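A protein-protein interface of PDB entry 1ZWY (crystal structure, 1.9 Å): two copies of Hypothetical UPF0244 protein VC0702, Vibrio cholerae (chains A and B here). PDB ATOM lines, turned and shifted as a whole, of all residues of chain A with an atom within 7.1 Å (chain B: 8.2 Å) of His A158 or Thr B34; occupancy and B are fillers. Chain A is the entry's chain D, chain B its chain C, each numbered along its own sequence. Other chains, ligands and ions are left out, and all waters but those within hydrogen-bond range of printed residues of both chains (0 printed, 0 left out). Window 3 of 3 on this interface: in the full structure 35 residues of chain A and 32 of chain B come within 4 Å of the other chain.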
ATOM      1  N   ILE A 151     -26.507  -1.760 -11.238  1.00  0.00           N
ATOM      2  CA  ILE A 151     -25.230  -2.462 -11.473  1.00  0.00           C
ATOM      3  C   ILE A 151     -24.952  -3.472 -10.369  1.00  0.00           C
ATOM      4  O   ILE A 151     -24.630  -4.618 -10.653  1.00  0.00           O
ATOM      5  CB  ILE A 151     -24.023  -1.529 -11.729  1.00  0.00           C
ATOM      6  CG1 ILE A 151     -24.098  -0.972 -13.146  1.00  0.00           C
ATOM      7  CG2 ILE A 151     -22.672  -2.317 -11.573  1.00  0.00           C
ATOM      8  CD1 ILE A 151     -23.243   0.318 -13.340  1.00  0.00           C
ATOM      9  N   GLY A 152     -25.126  -3.049  -9.113  1.00  0.00           N
ATOM     10  CA  GLY A 152     -25.043  -3.945  -7.959  1.00  0.00           C
ATOM     11  C   GLY A 152     -25.957  -5.158  -8.071  1.00  0.00           C
ATOM     12  O   GLY A 152     -25.542  -6.285  -7.837  1.00  0.00           O
ATOM     13  N   LEU A 154     -27.417  -6.510 -10.951  1.00  0.00           N
ATOM     14  CA  LEU A 154     -27.069  -7.319 -12.136  1.00  0.00           C
ATOM     15  C   LEU A 154     -25.727  -8.077 -12.059  1.00  0.00           C
ATOM     16  O   LEU A 154     -25.549  -9.116 -12.728  1.00  0.00           O
ATOM     17  CB  LEU A 154     -27.084  -6.435 -13.375  1.00  0.00           C
ATOM     18  CG  LEU A 154     -28.464  -5.892 -13.831  1.00  0.00           C
ATOM     19  CD1 LEU A 154     -28.306  -4.861 -14.967  1.00  0.00           C
ATOM     20  CD2 LEU A 154     -29.411  -7.027 -14.211  1.00  0.00           C
ATOM     21  N   THR A 155     -24.780  -7.568 -11.264  1.00  0.00           N
ATOM     22  CA  THR A 155     -23.482  -8.203 -11.173  1.00  0.00           C
ATOM     23  C   THR A 155     -23.309  -8.944  -9.827  1.00  0.00           C
ATOM     24  O   THR A 155     -22.179  -9.303  -9.467  1.00  0.00           O
ATOM     25  CB  THR A 155     -22.304  -7.186 -11.324  1.00  0.00           C
ATOM     26  OG1 THR A 155     -22.330  -6.274 -10.220  1.00  0.00           O
ATOM     27  CG2 THR A 155     -22.431  -6.361 -12.605  1.00  0.00           C
ATOM     28  N   ARG A 156     -24.405  -9.185  -9.097  1.00  0.00           N
ATOM     29  CA  ARG A 156     -24.312  -9.823  -7.770  1.00  0.00           C
ATOM     30  C   ARG A 156     -23.273  -9.133  -6.865  1.00  0.00           C
ATOM     31  O   ARG A 156     -22.452  -9.795  -6.211  1.00  0.00           O
ATOM     32  CB  ARG A 156     -23.989 -11.311  -7.892  1.00  0.00           C
ATOM     33  CG  ARG A 156     -25.055 -12.120  -8.613  1.00  0.00           C
ATOM     34  CD  ARG A 156     -24.602 -13.548  -8.677  1.00  0.00           C
ATOM     35  NE  ARG A 156     -25.438 -14.366  -9.554  1.00  0.00           N
ATOM     36  CZ  ARG A 156     -25.044 -15.541 -10.038  1.00  0.00           C
ATOM     37  NH1 ARG A 156     -23.825 -15.998  -9.741  1.00  0.00           N
ATOM     38  NH2 ARG A 156     -25.849 -16.250 -10.828  1.00  0.00           N
ATOM     39  N   HIS A 157     -23.325  -7.800  -6.850  1.00  0.00           N
ATOM     40  CA  HIS A 157     -22.465  -6.941  -6.036  1.00  0.00           C
ATOM     41  C   HIS A 157     -20.994  -6.935  -6.408  1.00  0.00           C
ATOM     42  O   HIS A 157     -20.203  -6.310  -5.714  1.00  0.00           O
ATOM     43  CB  HIS A 157     -22.580  -7.289  -4.551  1.00  0.00           C
ATOM     44  CG  HIS A 157     -23.987  -7.386  -4.053  1.00  0.00           C
ATOM     45  ND1 HIS A 157     -24.835  -6.303  -4.013  1.00  0.00           N
ATOM     46  CD2 HIS A 157     -24.688  -8.437  -3.563  1.00  0.00           C
ATOM     47  CE1 HIS A 157     -26.006  -6.682  -3.528  1.00  0.00           C
ATOM     48  NE2 HIS A 157     -25.944  -7.973  -3.247  1.00  0.00           N
ATOM     49  N   HIS A 158     -20.614  -7.623  -7.483  1.00  0.00           N
ATOM     50  CA  HIS A 158     -19.219  -7.584  -7.917  1.00  0.00           C
ATOM     51  C   HIS A 158     -18.802  -6.206  -8.379  1.00  0.00           C
ATOM     52  O   HIS A 158     -17.630  -5.844  -8.264  1.00  0.00           O
ATOM     53  CB  HIS A 158     -18.923  -8.635  -8.976  1.00  0.00           C
ATOM     54  CG  HIS A 158     -18.994 -10.031  -8.457  1.00  0.00           C
ATOM     55  ND1 HIS A 158     -18.224 -10.468  -7.400  1.00  0.00           N
ATOM     56  CD2 HIS A 158     -19.743 -11.093  -8.847  1.00  0.00           C
ATOM     57  CE1 HIS A 158     -18.515 -11.731  -7.145  1.00  0.00           C
ATOM     58  NE2 HIS A 158     -19.424 -12.136  -8.012  1.00  0.00           N
ATOM     59  N   LEU A 159     -19.757  -5.447  -8.917  1.00  0.00           N
ATOM     60  CA  LEU A 159     -19.561  -4.047  -9.196  1.00  0.00           C
ATOM     61  C   LEU A 159     -20.734  -3.274  -8.666  1.00  0.00           C
ATOM     62  O   LEU A 159     -21.815  -3.831  -8.429  1.00  0.00           O
ATOM     63  CB  LEU A 159     -19.462  -3.761 -10.705  1.00  0.00           C
ATOM     64  CG  LEU A 159     -18.366  -4.507 -11.459  1.00  0.00           C
ATOM     65  CD1 LEU A 159     -18.614  -4.390 -12.966  1.00  0.00           C
ATOM     66  CD2 LEU A 159     -16.972  -3.930 -11.059  1.00  0.00           C
ATOM     67  N   THR A 160     -20.509  -1.979  -8.557  1.00  0.00           N
ATOM     68  CA  THR A 160     -21.496  -1.010  -8.169  1.00  0.00           C
ATOM     69  C   THR A 160     -21.318   0.210  -9.118  1.00  0.00           C
ATOM     70  O   THR A 160     -20.246   0.407  -9.678  1.00  0.00           O
ATOM     71  CB  THR A 160     -21.180  -0.714  -6.707  1.00  0.00           C
ATOM     72  OG1 THR A 160     -22.194  -1.301  -5.864  1.00  0.00           O
ATOM     73  CG2 THR A 160     -21.012   0.656  -6.452  1.00  0.00           C
ATOM     74  N   THR A 163     -18.192   1.970  -7.885  1.00  0.00           N
ATOM     75  CA  THR A 163     -16.868   1.451  -8.194  1.00  0.00           C
ATOM     76  C   THR A 163     -16.515   1.554  -9.681  1.00  0.00           C
ATOM     77  O   THR A 163     -15.351   1.642 -10.049  1.00  0.00           O
ATOM     78  CB  THR A 163     -16.626   0.060  -7.682  1.00  0.00           C
ATOM     79  OG1 THR A 163     -17.577  -0.853  -8.246  1.00  0.00           O
ATOM     80  CG2 THR A 163     -16.699   0.067  -6.158  1.00  0.00           C
ATOM     81  N   ALA B  27      -7.076 -12.522 -17.902  1.00  0.00           N
ATOM     82  CA  ALA B  27      -8.205 -11.633 -17.605  1.00  0.00           C
ATOM     83  C   ALA B  27      -9.544 -12.381 -17.649  1.00  0.00           C
ATOM     84  O   ALA B  27     -10.377 -12.247 -16.732  1.00  0.00           O
ATOM     85  CB  ALA B  27      -8.227 -10.468 -18.581  1.00  0.00           C
ATOM     86  N   VAL B  28      -9.740 -13.194 -18.696  1.00  0.00           N
ATOM     87  CA  VAL B  28     -11.011 -13.908 -18.858  1.00  0.00           C
ATOM     88  C   VAL B  28     -11.170 -14.959 -17.757  1.00  0.00           C
ATOM     89  O   VAL B  28     -12.212 -15.070 -17.132  1.00  0.00           O
ATOM     90  CB  VAL B  28     -11.152 -14.506 -20.269  1.00  0.00           C
ATOM     91  CG1 VAL B  28     -12.434 -15.331 -20.378  1.00  0.00           C
ATOM     92  CG2 VAL B  28     -11.136 -13.365 -21.316  1.00  0.00           C
ATOM     93  N   ARG B  29     -10.099 -15.715 -17.491  1.00  0.00           N
ATOM     94  CA  ARG B  29     -10.136 -16.719 -16.427  1.00  0.00           C
ATOM     95  C   ARG B  29     -10.545 -16.077 -15.087  1.00  0.00           C
ATOM     96  O   ARG B  29     -11.392 -16.602 -14.332  1.00  0.00           O
ATOM     97  CB  ARG B  29      -8.746 -17.385 -16.306  1.00  0.00           C
ATOM     98  CG  ARG B  29      -8.673 -18.392 -15.163  1.00  0.00           C
ATOM     99  CD  ARG B  29      -7.249 -18.922 -14.955  1.00  0.00           C
ATOM    100  NE  ARG B  29      -6.919 -19.923 -15.976  1.00  0.00           N
ATOM    101  CZ  ARG B  29      -6.127 -19.692 -17.025  1.00  0.00           C
ATOM    102  NH1 ARG B  29      -5.553 -18.502 -17.185  1.00  0.00           N
ATOM    103  NH2 ARG B  29      -5.890 -20.663 -17.903  1.00  0.00           N
ATOM    104  N   SER B  30      -9.954 -14.923 -14.810  1.00  0.00           N
ATOM    105  CA  SER B  30     -10.241 -14.189 -13.579  1.00  0.00           C
ATOM    106  C   SER B  30     -11.690 -13.693 -13.442  1.00  0.00           C
ATOM    107  O   SER B  30     -12.280 -13.806 -12.351  1.00  0.00           O
ATOM    108  CB  SER B  30      -9.246 -13.046 -13.438  1.00  0.00           C
ATOM    109  OG  SER B  30      -9.596 -12.191 -12.371  1.00  0.00           O
ATOM    110  N   ALA B  31     -12.249 -13.147 -14.534  1.00  0.00           N
ATOM    111  CA  ALA B  31     -13.669 -12.710 -14.562  1.00  0.00           C
ATOM    112  C   ALA B  31     -14.568 -13.900 -14.314  1.00  0.00           C
ATOM    113  O   ALA B  31     -15.534 -13.817 -13.537  1.00  0.00           O
ATOM    114  CB  ALA B  31     -14.034 -12.043 -15.917  1.00  0.00           C
ATOM    115  N   PHE B  32     -14.268 -15.025 -14.956  1.00  0.00           N
ATOM    116  CA  PHE B  32     -15.110 -16.201 -14.729  1.00  0.00           C
ATOM    117  C   PHE B  32     -15.001 -16.760 -13.316  1.00  0.00           C
ATOM    118  O   PHE B  32     -16.017 -17.188 -12.789  1.00  0.00           O
ATOM    119  CB  PHE B  32     -14.896 -17.289 -15.780  1.00  0.00           C
ATOM    120  CG  PHE B  32     -15.668 -17.052 -17.045  1.00  0.00           C
ATOM    121  CD1 PHE B  32     -15.194 -16.145 -18.009  1.00  0.00           C
ATOM    122  CD2 PHE B  32     -16.900 -17.678 -17.251  1.00  0.00           C
ATOM    123  CE1 PHE B  32     -15.939 -15.916 -19.194  1.00  0.00           C
ATOM    124  CE2 PHE B  32     -17.611 -17.487 -18.410  1.00  0.00           C
ATOM    125  CZ  PHE B  32     -17.144 -16.585 -19.382  1.00  0.00           C
ATOM    126  N   SER B  33     -13.801 -16.756 -12.715  1.00  0.00           N
ATOM    127  CA  SER B  33     -13.652 -17.231 -11.312  1.00  0.00           C
ATOM    128  C   SER B  33     -14.415 -16.350 -10.326  1.00  0.00           C
ATOM    129  O   SER B  33     -14.978 -16.849  -9.355  1.00  0.00           O
ATOM    130  CB  SER B  33     -12.191 -17.286 -10.868  1.00  0.00           C
ATOM    131  OG  SER B  33     -11.352 -17.645 -11.945  1.00  0.00           O
ATOM    132  N   THR B  34     -14.421 -15.036 -10.578  1.00  0.00           N
ATOM    133  CA  THR B  34     -15.144 -14.099  -9.726  1.00  0.00           C
ATOM    134  C   THR B  34     -16.665 -14.329  -9.765  1.00  0.00           C
ATOM    135  O   THR B  34     -17.334 -14.421  -8.737  1.00  0.00           O
ATOM    136  CB  THR B  34     -14.835 -12.642 -10.124  1.00  0.00           C
ATOM    137  OG1 THR B  34     -13.467 -12.347  -9.846  1.00  0.00           O
ATOM    138  CG2 THR B  34     -15.690 -11.666  -9.315  1.00  0.00           C
ATOM    139  N   VAL B  35     -17.221 -14.377 -10.954  1.00  0.00           N
ATOM    140  CA  VAL B  35     -18.675 -14.385 -11.027  1.00  0.00           C
ATOM    141  C   VAL B  35     -19.248 -15.787 -10.885  1.00  0.00           C
ATOM    142  O   VAL B  35     -20.333 -15.943 -10.332  1.00  0.00           O
ATOM    143  CB  VAL B  35     -19.213 -13.633 -12.258  1.00  0.00           C
ATOM    144  CG1 VAL B  35     -18.832 -12.159 -12.186  1.00  0.00           C
ATOM    145  CG2 VAL B  35     -18.700 -14.272 -13.509  1.00  0.00           C
ATOM    146  N   PHE B  36     -18.499 -16.807 -11.301  1.00  0.00           N
ATOM    147  CA  PHE B  36     -18.945 -18.195 -11.146  1.00  0.00           C
ATOM    148  C   PHE B  36     -17.925 -18.994 -10.325  1.00  0.00           C
ATOM    149  O   PHE B  36     -17.252 -19.866 -10.880  1.00  0.00           O
ATOM    150  CB  PHE B  36     -19.107 -18.839 -12.509  1.00  0.00           C
ATOM    151  CG  PHE B  36     -19.998 -18.075 -13.448  1.00  0.00           C
ATOM    152  CD1 PHE B  36     -21.370 -17.945 -13.179  1.00  0.00           C
ATOM    153  CD2 PHE B  36     -19.478 -17.545 -14.630  1.00  0.00           C
ATOM    154  CE1 PHE B  36     -22.223 -17.253 -14.066  1.00  0.00           C
ATOM    155  CE2 PHE B  36     -20.313 -16.862 -15.535  1.00  0.00           C
ATOM    156  CZ  PHE B  36     -21.699 -16.717 -15.254  1.00  0.00           C
ATOM    157  N   PRO B  37     -17.794 -18.682  -9.017  1.00  0.00           N
ATOM    158  CA  PRO B  37     -16.702 -19.235  -8.184  1.00  0.00           C
ATOM    159  C   PRO B  37     -16.729 -20.761  -7.986  1.00  0.00           C
ATOM    160  O   PRO B  37     -15.691 -21.356  -7.641  1.00  0.00           O
ATOM    161  CB  PRO B  37     -16.902 -18.530  -6.835  1.00  0.00           C
ATOM    162  CG  PRO B  37     -18.324 -18.138  -6.812  1.00  0.00           C
ATOM    163  CD  PRO B  37     -18.645 -17.769  -8.236  1.00  0.00           C
ATOM    164  N   ASP B  38     -17.903 -21.359  -8.181  1.00  0.00           N
ATOM    165  CA  ASP B  38     -18.133 -22.798  -7.975  1.00  0.00           C
ATOM    166  C   ASP B  38     -17.962 -23.631  -9.246  1.00  0.00           C
ATOM    167  O   ASP B  38     -18.169 -24.851  -9.220  1.00  0.00           O
ATOM    168  CB  ASP B  38     -19.555 -23.045  -7.460  1.00  0.00           C
ATOM    169  CG  ASP B  38     -19.811 -22.431  -6.095  1.00  0.00           C
ATOM    170  OD1 ASP B  38     -18.912 -22.475  -5.226  1.00  0.00           O
ATOM    171  OD2 ASP B  38     -20.939 -21.926  -5.891  1.00  0.00           O
ATOM    172  N   GLN B  39     -17.605 -22.991 -10.353  1.00  0.00           N
ATOM    173  CA  GLN B  39     -17.509 -23.702 -11.622  1.00  0.00           C
ATOM    174  C   GLN B  39     -16.071 -23.792 -12.150  1.00  0.00           C
ATOM    175  O   GLN B  39     -15.198 -23.047 -11.726  1.00  0.00           O
ATOM    176  CB  GLN B  39     -18.480 -23.085 -12.651  1.00  0.00           C
ATOM    177  CG  GLN B  39     -19.952 -23.457 -12.397  1.00  0.00           C
ATOM    178  CD  GLN B  39     -20.923 -22.370 -12.803  1.00  0.00           C
ATOM    179  OE1 GLN B  39     -21.344 -22.292 -13.959  1.00  0.00           O
ATOM    180  NE2 GLN B  39     -21.292 -21.522 -11.848  1.00  0.00           N
ATOM    181  N   TRP B  41     -13.628 -24.386 -15.817  1.00  0.00           N
ATOM    182  CA  TRP B  41     -13.542 -24.480 -17.276  1.00  0.00           C
ATOM    183  C   TRP B  41     -12.105 -24.690 -17.714  1.00  0.00           C
ATOM    184  O   TRP B  41     -11.184 -24.346 -16.972  1.00  0.00           O
ATOM    185  CB  TRP B  41     -14.059 -23.188 -17.928  1.00  0.00           C
ATOM    186  CG  TRP B  41     -15.532 -23.021 -17.859  1.00  0.00           C
ATOM    187  CD1 TRP B  41     -16.457 -23.542 -18.722  1.00  0.00           C
ATOM    188  CD2 TRP B  41     -16.262 -22.264 -16.895  1.00  0.00           C
ATOM    189  NE1 TRP B  41     -17.719 -23.160 -18.352  1.00  0.00           N
ATOM    190  CE2 TRP B  41     -17.633 -22.371 -17.235  1.00  0.00           C
ATOM    191  CE3 TRP B  41     -15.894 -21.492 -15.783  1.00  0.00           C
ATOM    192  CZ2 TRP B  41     -18.632 -21.760 -16.498  1.00  0.00           C
ATOM    193  CZ3 TRP B  41     -16.892 -20.874 -15.046  1.00  0.00           C
ATOM    194  CH2 TRP B  41     -18.251 -21.007 -15.412  1.00  0.00           C
ATOM    195  N   HIS B 166     -11.105  -6.185 -15.897  1.00  0.00           N
ATOM    196  CA  HIS B 166     -11.920  -7.024 -15.004  1.00  0.00           C
ATOM    197  C   HIS B 166     -13.326  -6.450 -14.939  1.00  0.00           C
ATOM    198  O   HIS B 166     -14.301  -7.203 -15.031  1.00  0.00           O
ATOM    199  CB  HIS B 166     -11.306  -7.061 -13.609  1.00  0.00           C
ATOM    200  CG  HIS B 166     -11.877  -8.116 -12.689  1.00  0.00           C
ATOM    201  ND1 HIS B 166     -11.803  -9.468 -12.954  1.00  0.00           N
ATOM    202  CD2 HIS B 166     -12.465  -8.006 -11.471  1.00  0.00           C
ATOM    203  CE1 HIS B 166     -12.350 -10.144 -11.953  1.00  0.00           C
ATOM    204  NE2 HIS B 166     -12.754  -9.283 -11.038  1.00  0.00           N
ATOM    205  N   GLN B 167     -13.434  -5.126 -14.798  1.00  0.00           N
ATOM    206  CA  GLN B 167     -14.749  -4.497 -14.708  1.00  0.00           C
ATOM    207  C   GLN B 167     -15.577  -4.708 -15.987  1.00  0.00           C
ATOM    208  O   GLN B 167     -16.761  -5.041 -15.914  1.00  0.00           O
ATOM    209  CB  GLN B 167     -14.629  -2.985 -14.363  1.00  0.00           C
ATOM    210  CG  GLN B 167     -14.187  -2.772 -12.927  1.00  0.00           C
ATOM    211  CD  GLN B 167     -14.644  -1.459 -12.306  1.00  0.00           C
ATOM    212  OE1 GLN B 167     -15.198  -0.593 -12.988  1.00  0.00           O
ATOM    213  NE2 GLN B 167     -14.429  -1.323 -10.983  1.00  0.00           N
ATOM    214  N   ILE B 170     -16.738  -8.372 -16.306  1.00  0.00           N
ATOM    215  CA  ILE B 170     -17.887  -8.623 -15.416  1.00  0.00           C
ATOM    216  C   ILE B 170     -19.175  -8.012 -16.015  1.00  0.00           C
ATOM    217  O   ILE B 170     -20.206  -8.654 -16.005  1.00  0.00           O
ATOM    218  CB  ILE B 170     -17.658  -8.047 -13.998  1.00  0.00           C
ATOM    219  CG1 ILE B 170     -16.581  -8.873 -13.262  1.00  0.00           C
ATOM    220  CG2 ILE B 170     -18.981  -8.095 -13.199  1.00  0.00           C
ATOM    221  CD1 ILE B 170     -16.030  -8.227 -11.923  1.00  0.00           C
ATOM    222  N   LEU B 171     -19.110  -6.761 -16.486  1.00  0.00           N
ATOM    223  CA  LEU B 171     -20.299  -6.124 -17.105  1.00  0.00           C
ATOM    224  C   LEU B 171     -20.752  -6.940 -18.315  1.00  0.00           C
ATOM    225  O   LEU B 171     -21.936  -7.075 -18.557  1.00  0.00           O
ATOM    226  CB  LEU B 171     -20.000  -4.672 -17.512  1.00  0.00           C
ATOM    227  CG  LEU B 171     -19.844  -3.686 -16.339  1.00  0.00           C
ATOM    228  CD1 LEU B 171     -19.231  -2.322 -16.814  1.00  0.00           C
ATOM    229  CD2 LEU B 171     -21.150  -3.460 -15.559  1.00  0.00           C
ATOM    230  N   LEU B 173     -20.640 -10.061 -18.619  1.00  0.00           N
ATOM    231  CA  LEU B 173     -21.229 -11.311 -18.189  1.00  0.00           C
ATOM    232  C   LEU B 173     -22.655 -11.153 -17.665  1.00  0.00           C
ATOM    233  O   LEU B 173     -23.294 -12.123 -17.325  1.00  0.00           O
ATOM    234  CB  LEU B 173     -20.346 -12.009 -17.113  1.00  0.00           C
ATOM    235  CG  LEU B 173     -19.047 -12.643 -17.613  1.00  0.00           C
ATOM    236  CD1 LEU B 173     -18.134 -13.109 -16.445  1.00  0.00           C
ATOM    237  CD2 LEU B 173     -19.408 -13.832 -18.502  1.00  0.00           C
ATOM    238  N   ILE B 177     -25.574 -13.921 -16.047  1.00  0.00           N
ATOM    239  CA  ILE B 177     -25.925 -13.820 -14.634  1.00  0.00           C
ATOM    240  C   ILE B 177     -27.461 -13.670 -14.512  1.00  0.00           C
ATOM    241  O   ILE B 177     -28.059 -14.156 -13.557  1.00  0.00           O
ATOM    242  CB  ILE B 177     -25.188 -12.606 -13.973  1.00  0.00           C
ATOM    243  CG1 ILE B 177     -23.683 -12.830 -13.897  1.00  0.00           C
ATOM    244  CG2 ILE B 177     -25.685 -12.321 -12.544  1.00  0.00           C
ATOM    245  CD1 ILE B 177     -22.917 -11.610 -13.445  1.00  0.00           C
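A ring nitrogen (NE2) of His A158 sits at hydrogen-bond distance from the backbone carbonyl oxygen (O) of Thr B34 (3.2 Å).
NE2 of Gln B167 sits at hydrogen-bond distance from O of Thr A163 (3.2 Å).
O of Ser B30 lies within hydrogen-bond range of OG1 of Thr B34 (3.1 Å).
The side-chain hydroxyl of Thr B34 sits close to a ring nitrogen (NE2) of His B166 (3.4 Å).
The backbone carbonyl oxygen (O) of Ile A151 lies within hydrogen-bond range of the side-chain hydroxyl (OG1) of Thr A155.
The backbone NH of Gly A152 lies close to the backbone carbonyl oxygen of Leu A159, 3.5 Å away.
The side-chain hydroxyl of Thr A155 lies within hydrogen-bond range of the backbone NH of Leu A159, at 3.0 Å.
N of Thr A160 is in hydrogen-bond range of OG1 of Thr A163.
Leu A154 touches Ile B177.
Thr A155 touches Ile B170 (CG2 to CG2, 3.9 Å).
NH1 of Arg A156 touches O of Val B35, at 3.5 Å.
Ile B177 touches Arg A156.
CD2 of His A158 touches CG1 of Val B35 (3.6 Å).
CD1 of Leu A159 touches O of Gln B167, 3.5 Å away.
Leu A159 touches Ile B170.
Leu B171 touches Leu A159 (CG to CD1, 3.7 Å).
Of the printed residues of chain B, Arg A156 touches Val B35 and Ile B177.
Of the printed residues of chain B, His A158 touches Thr B34 (3.2 Å) and Val B35 (3.6 Å).
Printed residues of chain B within 4 Å of Leu A159: Gln B167 (3.5 Å), Ile B170 (3.7 Å) and Leu B171 (3.7 Å).
Thr B34 touches just one residue of chain A: His A158 (3.2 Å).
Of the printed residues of chain A, Val B35 touches Arg A156 (3.5 Å) and His A158 (3.6 Å).
Printed residues of chain A within 4 Å of Gln B167: Leu A159 (3.5 Å) and Thr A163 (3.2 Å).
Of the printed residues of chain A, Ile B177 touches Leu A154 and Arg A156.
Hydrophobic or aromatic side chains of chain A that line the printed part of chain B: His A158 and Leu A159.
Hydrophobic or aromatic side chains of chain B within 4 Å of the printed part of chain A: Val B35, Ile B170, Leu B171 and Ile B177.
Among the printed residues, no Asp or Glu carboxylate lies within 4 Å of a Lys or Arg side-chain nitrogen of the other chain.
No position is printed for both chains.
Of the 10 pairs that touch across the chains among the printed residues, none has its exchanged pair printed and touching as well.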
